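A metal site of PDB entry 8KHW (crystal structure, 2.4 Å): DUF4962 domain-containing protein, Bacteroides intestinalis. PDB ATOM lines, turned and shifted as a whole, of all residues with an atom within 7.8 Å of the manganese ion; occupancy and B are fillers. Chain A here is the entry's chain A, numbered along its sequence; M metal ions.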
ATOM      1  N   ASN A 277      -5.148  -2.857  14.494  1.00  0.00           N
ATOM      2  CA  ASN A 277      -4.192  -3.886  14.058  1.00  0.00           C
ATOM      3  C   ASN A 277      -4.585  -4.475  12.698  1.00  0.00           C
ATOM      4  O   ASN A 277      -4.720  -5.699  12.516  1.00  0.00           O
ATOM      5  CB  ASN A 277      -4.097  -4.972  15.122  1.00  0.00           C
ATOM      6  CG  ASN A 277      -5.448  -5.666  15.371  1.00  0.00           C
ATOM      7  OD1 ASN A 277      -6.512  -5.025  15.317  1.00  0.00           O
ATOM      8  ND2 ASN A 277      -5.407  -6.968  15.592  1.00  0.00           N
ATOM      9  N   TYR A 278      -4.741  -3.607  11.710  1.00  0.00           N
ATOM     10  CA  TYR A 278      -4.985  -4.137  10.380  1.00  0.00           C
ATOM     11  C   TYR A 278      -3.688  -4.713   9.814  1.00  0.00           C
ATOM     12  O   TYR A 278      -2.592  -4.391  10.281  1.00  0.00           O
ATOM     13  CB  TYR A 278      -5.573  -3.051   9.479  1.00  0.00           C
ATOM     14  CG  TYR A 278      -4.675  -1.870   9.181  1.00  0.00           C
ATOM     15  CD1 TYR A 278      -3.552  -2.025   8.360  1.00  0.00           C
ATOM     16  CD2 TYR A 278      -4.972  -0.596   9.670  1.00  0.00           C
ATOM     17  CE1 TYR A 278      -2.744  -0.969   8.067  1.00  0.00           C
ATOM     18  CE2 TYR A 278      -4.163   0.480   9.382  1.00  0.00           C
ATOM     19  CZ  TYR A 278      -3.035   0.290   8.573  1.00  0.00           C
ATOM     20  OH  TYR A 278      -2.199   1.334   8.248  1.00  0.00           O
ATOM     21  N   GLY A 279      -3.821  -5.605   8.835  1.00  0.00           N
ATOM     22  CA  GLY A 279      -2.744  -6.367   8.252  1.00  0.00           C
ATOM     23  C   GLY A 279      -1.905  -7.095   9.293  1.00  0.00           C
ATOM     24  O   GLY A 279      -2.400  -7.561  10.325  1.00  0.00           O
ATOM     25  N   ASP A 280      -0.605  -7.177   9.037  1.00  0.00           N
ATOM     26  CA  ASP A 280       0.193  -7.992   9.949  1.00  0.00           C
ATOM     27  C   ASP A 280       0.542  -7.297  11.271  1.00  0.00           C
ATOM     28  O   ASP A 280       1.318  -7.853  12.042  1.00  0.00           O
ATOM     29  CB  ASP A 280       1.447  -8.493   9.233  1.00  0.00           C
ATOM     30  CG  ASP A 280       1.109  -9.478   8.124  1.00  0.00           C
ATOM     31  OD1 ASP A 280      -0.026 -10.036   8.163  1.00  0.00           O
ATOM     32  OD2 ASP A 280       1.956  -9.685   7.225  1.00  0.00           O
ATOM     33  N   CYS A 281      -0.060  -6.155  11.599  1.00  0.00           N
ATOM     34  CA  CYS A 281       0.211  -5.499  12.884  1.00  0.00           C
ATOM     35  C   CYS A 281      -0.261  -6.339  14.061  1.00  0.00           C
ATOM     36  O   CYS A 281      -1.195  -7.134  13.960  1.00  0.00           O
ATOM     37  CB  CYS A 281      -0.473  -4.134  12.949  1.00  0.00           C
ATOM     38  SG  CYS A 281       0.246  -2.916  11.808  1.00  0.00           S
ATOM     39  N   LYS A 375     -10.960   1.585   7.519  1.00  0.00           N
ATOM     40  CA  LYS A 375      -9.843   1.562   6.602  1.00  0.00           C
ATOM     41  C   LYS A 375     -10.162   1.199   5.170  1.00  0.00           C
ATOM     42  O   LYS A 375     -10.914   0.264   4.919  1.00  0.00           O
ATOM     43  CB  LYS A 375      -8.756   0.605   7.104  1.00  0.00           C
ATOM     44  CG  LYS A 375      -9.222  -0.837   7.287  1.00  0.00           C
ATOM     45  CD  LYS A 375      -8.139  -1.825   6.912  1.00  0.00           C
ATOM     46  CE  LYS A 375      -6.946  -1.093   6.330  1.00  0.00           C
ATOM     47  NZ  LYS A 375      -6.412  -1.773   5.115  1.00  0.00           N
ATOM     48  N   HIS A 383       2.323  -6.112   3.912  1.00  0.00           N
ATOM     49  CA  HIS A 383       1.677  -6.699   5.095  1.00  0.00           C
ATOM     50  C   HIS A 383       0.155  -6.499   5.104  1.00  0.00           C
ATOM     51  O   HIS A 383      -0.435  -6.147   6.129  1.00  0.00           O
ATOM     52  CB  HIS A 383       2.303  -6.173   6.395  1.00  0.00           C
ATOM     53  CG  HIS A 383       3.710  -6.606   6.595  1.00  0.00           C
ATOM     54  ND1 HIS A 383       4.061  -7.907   6.888  1.00  0.00           N
ATOM     55  CD2 HIS A 383       4.880  -5.915   6.522  1.00  0.00           C
ATOM     56  CE1 HIS A 383       5.370  -8.002   7.003  1.00  0.00           C
ATOM     57  NE2 HIS A 383       5.892  -6.799   6.777  1.00  0.00           N
ATOM     58  N   THR A 384      -0.474  -6.774   3.986  1.00  0.00           N
ATOM     59  CA  THR A 384      -1.904  -6.525   3.851  1.00  0.00           C
ATOM     60  C   THR A 384      -2.755  -7.767   4.141  1.00  0.00           C
ATOM     61  O   THR A 384      -2.332  -8.899   3.904  1.00  0.00           O
ATOM     62  CB  THR A 384      -2.211  -6.043   2.445  1.00  0.00           C
ATOM     63  OG1 THR A 384      -1.634  -6.977   1.535  1.00  0.00           O
ATOM     64  CG2 THR A 384      -1.592  -4.675   2.247  1.00  0.00           C
ATOM     65  N   HIS A 385      -3.963  -7.525   4.630  1.00  0.00           N
ATOM     66  CA  HIS A 385      -5.041  -8.494   4.569  1.00  0.00           C
ATOM     67  C   HIS A 385      -6.110  -7.996   3.593  1.00  0.00           C
ATOM     68  O   HIS A 385      -6.138  -6.821   3.233  1.00  0.00           O
ATOM     69  CB  HIS A 385      -5.664  -8.724   5.957  1.00  0.00           C
ATOM     70  CG  HIS A 385      -4.697  -9.262   6.977  1.00  0.00           C
ATOM     71  ND1 HIS A 385      -5.041  -9.459   8.290  1.00  0.00           N
ATOM     72  CD2 HIS A 385      -3.406  -9.654   6.860  1.00  0.00           C
ATOM     73  CE1 HIS A 385      -4.011  -9.949   8.951  1.00  0.00           C
ATOM     74  NE2 HIS A 385      -2.999 -10.072   8.104  1.00  0.00           N
ATOM     75  N   LEU A 386      -6.997  -8.898   3.169  1.00  0.00           N
ATOM     76  CA  LEU A 386      -8.139  -8.503   2.344  1.00  0.00           C
ATOM     77  C   LEU A 386      -9.196  -7.875   3.251  1.00  0.00           C
ATOM     78  O   LEU A 386     -10.209  -8.481   3.626  1.00  0.00           O
ATOM     79  CB  LEU A 386      -8.672  -9.685   1.546  1.00  0.00           C
ATOM     80  CG  LEU A 386      -7.615 -10.328   0.620  1.00  0.00           C
ATOM     81  CD1 LEU A 386      -8.204 -11.309  -0.402  1.00  0.00           C
ATOM     82  CD2 LEU A 386      -6.801  -9.254  -0.101  1.00  0.00           C
ATOM     83  N   ASP A 387      -8.959  -6.610   3.604  1.00  0.00           N
ATOM     84  CA  ASP A 387      -9.715  -5.964   4.668  1.00  0.00           C
ATOM     85  C   ASP A 387     -10.187  -4.569   4.279  1.00  0.00           C
ATOM     86  O   ASP A 387     -10.521  -3.768   5.154  1.00  0.00           O
ATOM     87  CB  ASP A 387      -8.873  -5.908   5.954  1.00  0.00           C
ATOM     88  CG  ASP A 387      -7.523  -5.222   5.733  1.00  0.00           C
ATOM     89  OD1 ASP A 387      -7.378  -4.463   4.733  1.00  0.00           O
ATOM     90  OD2 ASP A 387      -6.614  -5.432   6.556  1.00  0.00           O
ATOM     91  N   SER A 390     -12.871  -2.636   6.187  1.00  0.00           N
ATOM     92  CA  SER A 390     -12.976  -3.200   7.523  1.00  0.00           C
ATOM     93  C   SER A 390     -12.991  -2.080   8.561  1.00  0.00           C
ATOM     94  O   SER A 390     -12.446  -0.996   8.346  1.00  0.00           O
ATOM     95  CB  SER A 390     -11.804  -4.158   7.800  1.00  0.00           C
ATOM     96  OG  SER A 390     -12.168  -5.077   8.805  1.00  0.00           O
ATOM     97  N   THR A 402     -13.510  -6.899  16.052  1.00  0.00           N
ATOM     98  CA  THR A 402     -12.057  -6.980  16.103  1.00  0.00           C
ATOM     99  C   THR A 402     -11.484  -7.465  14.783  1.00  0.00           C
ATOM    100  O   THR A 402     -12.198  -7.786  13.832  1.00  0.00           O
ATOM    101  CB  THR A 402     -11.596  -7.924  17.216  1.00  0.00           C
ATOM    102  OG1 THR A 402     -11.957  -9.258  16.860  1.00  0.00           O
ATOM    103  CG2 THR A 402     -12.229  -7.556  18.515  1.00  0.00           C
ATOM    104  N   ASP A 403     -10.149  -7.537  14.781  1.00  0.00           N
ATOM    105  CA  ASP A 403      -9.350  -8.039  13.679  1.00  0.00           C
ATOM    106  C   ASP A 403      -8.403  -9.098  14.227  1.00  0.00           C
ATOM    107  O   ASP A 403      -7.663  -8.830  15.179  1.00  0.00           O
ATOM    108  CB  ASP A 403      -8.549  -6.908  13.017  1.00  0.00           C
ATOM    109  CG  ASP A 403      -8.083  -7.256  11.628  1.00  0.00           C
ATOM    110  OD1 ASP A 403      -8.015  -8.458  11.313  1.00  0.00           O
ATOM    111  OD2 ASP A 403      -7.797  -6.334  10.842  1.00  0.00           O
ATOM    112  N   LEU A 404      -8.411 -10.287  13.617  1.00  0.00           N
ATOM    113  CA  LEU A 404      -7.628 -11.405  14.135  1.00  0.00           C
ATOM    114  C   LEU A 404      -6.122 -11.115  14.124  1.00  0.00           C
ATOM    115  O   LEU A 404      -5.383 -11.699  14.923  1.00  0.00           O
ATOM    116  CB  LEU A 404      -7.916 -12.665  13.332  1.00  0.00           C
ATOM    117  CG  LEU A 404      -9.330 -13.216  13.486  1.00  0.00           C
ATOM    118  CD1 LEU A 404      -9.395 -14.534  12.750  1.00  0.00           C
ATOM    119  CD2 LEU A 404      -9.727 -13.389  14.943  1.00  0.00           C
ATOM    120  N   GLY A 405      -5.658 -10.237  13.252  1.00  0.00           N
ATOM    121  CA  GLY A 405      -4.250  -9.994  13.121  1.00  0.00           C
ATOM    122  C   GLY A 405      -3.557 -11.116  12.383  1.00  0.00           C
ATOM    123  O   GLY A 405      -4.202 -11.977  11.752  1.00  0.00           O
ATOM    124  N   PRO A 406      -2.230 -11.147  12.457  1.00  0.00           N
ATOM    125  CA  PRO A 406      -1.441 -12.057  11.622  1.00  0.00           C
ATOM    126  C   PRO A 406      -1.456 -13.479  12.160  1.00  0.00           C
ATOM    127  O   PRO A 406      -1.883 -13.764  13.282  1.00  0.00           O
ATOM    128  CB  PRO A 406      -0.032 -11.464  11.685  1.00  0.00           C
ATOM    129  CG  PRO A 406       0.049 -10.884  13.074  1.00  0.00           C
ATOM    130  CD  PRO A 406      -1.391 -10.473  13.470  1.00  0.00           C
ATOM    131  N   ARG A 433      -6.767 -16.262   8.264  1.00  0.00           N
ATOM    132  CA  ARG A 433      -6.762 -14.942   8.888  1.00  0.00           C
ATOM    133  C   ARG A 433      -6.581 -13.788   7.920  1.00  0.00           C
ATOM    134  O   ARG A 433      -6.627 -12.636   8.370  1.00  0.00           O
ATOM    135  CB  ARG A 433      -5.672 -14.864   9.955  1.00  0.00           C
ATOM    136  CG  ARG A 433      -6.128 -15.344  11.330  1.00  0.00           C
ATOM    137  CD  ARG A 433      -4.962 -15.361  12.322  1.00  0.00           C
ATOM    138  NE  ARG A 433      -5.349 -15.945  13.612  1.00  0.00           N
ATOM    139  CZ  ARG A 433      -4.492 -16.267  14.578  1.00  0.00           C
ATOM    140  NH1 ARG A 433      -3.189 -16.058  14.396  1.00  0.00           N
ATOM    141  NH2 ARG A 433      -4.936 -16.804  15.709  1.00  0.00           N
ATOM    142  N   TYR A 434      -6.411 -14.038   6.621  1.00  0.00           N
ATOM    143  CA  TYR A 434      -5.953 -13.017   5.686  1.00  0.00           C
ATOM    144  C   TYR A 434      -6.968 -12.601   4.629  1.00  0.00           C
ATOM    145  O   TYR A 434      -6.752 -11.594   3.953  1.00  0.00           O
ATOM    146  CB  TYR A 434      -4.676 -13.484   4.959  1.00  0.00           C
ATOM    147  CG  TYR A 434      -3.453 -13.576   5.843  1.00  0.00           C
ATOM    148  CD1 TYR A 434      -3.427 -14.428   6.934  1.00  0.00           C
ATOM    149  CD2 TYR A 434      -2.303 -12.825   5.566  1.00  0.00           C
ATOM    150  CE1 TYR A 434      -2.322 -14.536   7.743  1.00  0.00           C
ATOM    151  CE2 TYR A 434      -1.164 -12.947   6.380  1.00  0.00           C
ATOM    152  CZ  TYR A 434      -1.188 -13.799   7.476  1.00  0.00           C
ATOM    153  OH  TYR A 434      -0.122 -13.948   8.323  1.00  0.00           O
ATOM    154  N   ASN A 435      -8.040 -13.364   4.428  1.00  0.00           N
ATOM    155  CA  ASN A 435      -9.021 -12.986   3.429  1.00  0.00           C
ATOM    156  C   ASN A 435     -10.234 -12.350   4.103  1.00  0.00           C
ATOM    157  O   ASN A 435     -10.362 -12.351   5.326  1.00  0.00           O
ATOM    158  CB  ASN A 435      -9.419 -14.194   2.563  1.00  0.00           C
ATOM    159  CG  ASN A 435      -9.990 -15.323   3.375  1.00  0.00           C
ATOM    160  OD1 ASN A 435     -11.029 -15.177   3.999  1.00  0.00           O
ATOM    161  ND2 ASN A 435      -9.320 -16.470   3.349  1.00  0.00           N
ATOM    162  N   ALA A 438     -12.907 -13.331   6.967  1.00  0.00           N
ATOM    163  CA  ALA A 438     -12.566 -13.318   8.382  1.00  0.00           C
ATOM    164  C   ALA A 438     -12.292 -11.904   8.904  1.00  0.00           C
ATOM    165  O   ALA A 438     -11.637 -11.758   9.928  1.00  0.00           O
ATOM    166  CB  ALA A 438     -11.356 -14.213   8.656  1.00  0.00           C
ATOM    167  N   HIS A 439     -12.768 -10.869   8.207  1.00  0.00           N
ATOM    168  CA  HIS A 439     -12.635  -9.487   8.670  1.00  0.00           C
ATOM    169  C   HIS A 439     -14.009  -8.804   8.616  1.00  0.00           C
ATOM    170  O   HIS A 439     -14.945  -9.306   7.994  1.00  0.00           O
ATOM    171  CB  HIS A 439     -11.637  -8.700   7.808  1.00  0.00           C
ATOM    172  CG  HIS A 439     -10.237  -9.184   7.927  1.00  0.00           C
ATOM    173  ND1 HIS A 439      -9.815 -10.378   7.400  1.00  0.00           N
ATOM    174  CD2 HIS A 439      -9.157  -8.632   8.539  1.00  0.00           C
ATOM    175  CE1 HIS A 439      -8.520 -10.545   7.663  1.00  0.00           C
ATOM    176  NE2 HIS A 439      -8.102  -9.494   8.346  1.00  0.00           N
ATOM    177  N   ASN A 440     -14.093  -7.623   9.226  1.00  0.00           N
ATOM    178  CA  ASN A 440     -15.371  -6.901   9.349  1.00  0.00           C
ATOM    179  C   ASN A 440     -15.714  -6.150   8.062  1.00  0.00           C
ATOM    180  O   ASN A 440     -15.863  -4.921   8.036  1.00  0.00           O
ATOM    181  CB  ASN A 440     -15.327  -5.963  10.543  1.00  0.00           C
ATOM    182  CG  ASN A 440     -14.825  -6.652  11.780  1.00  0.00           C
ATOM    183  OD1 ASN A 440     -15.154  -7.822  12.017  1.00  0.00           O
ATOM    184  ND2 ASN A 440     -13.993  -5.958  12.577  1.00  0.00           N
HETATM  185 MN    MN M   1      -6.489  -8.783   9.547  1.00  0.00          MN
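Within 4 Å of the manganese ion: His 385, Asp 403 and His 439.
The backbone carbonyl oxygen (O) of Gly 279 lies close to a ring nitrogen (NE2) of His 385 (3.4 Å). A ring nitrogen (NE2) of His 385 lies within hydrogen-bond range of the side-chain carboxylate (OD1) of Asp 280, at 3.0 Å. A ring nitrogen (NE2) of His 439 sits close to the backbone carbonyl oxygen (O) of Arg 433 (3.5 Å). The backbone carbonyl oxygen of Asn 435 is in hydrogen-bond range of a ring nitrogen (ND1) of His 439 (2.9 Å). The backbone carbonyl oxygen of Asp 403 lies within hydrogen-bond range of the side-chain amide nitrogen of Asn 277 (3.0 Å).
The manganese ion is bound by a ring nitrogen (ND1) of His 385 (2.0 Å), a ring nitrogen (NE2) of His 439 (2.1 Å) and the side-chain carboxylate (OD1) of Asp 403 (2.4 Å). The manganese ion has three donor atoms within binding distance.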
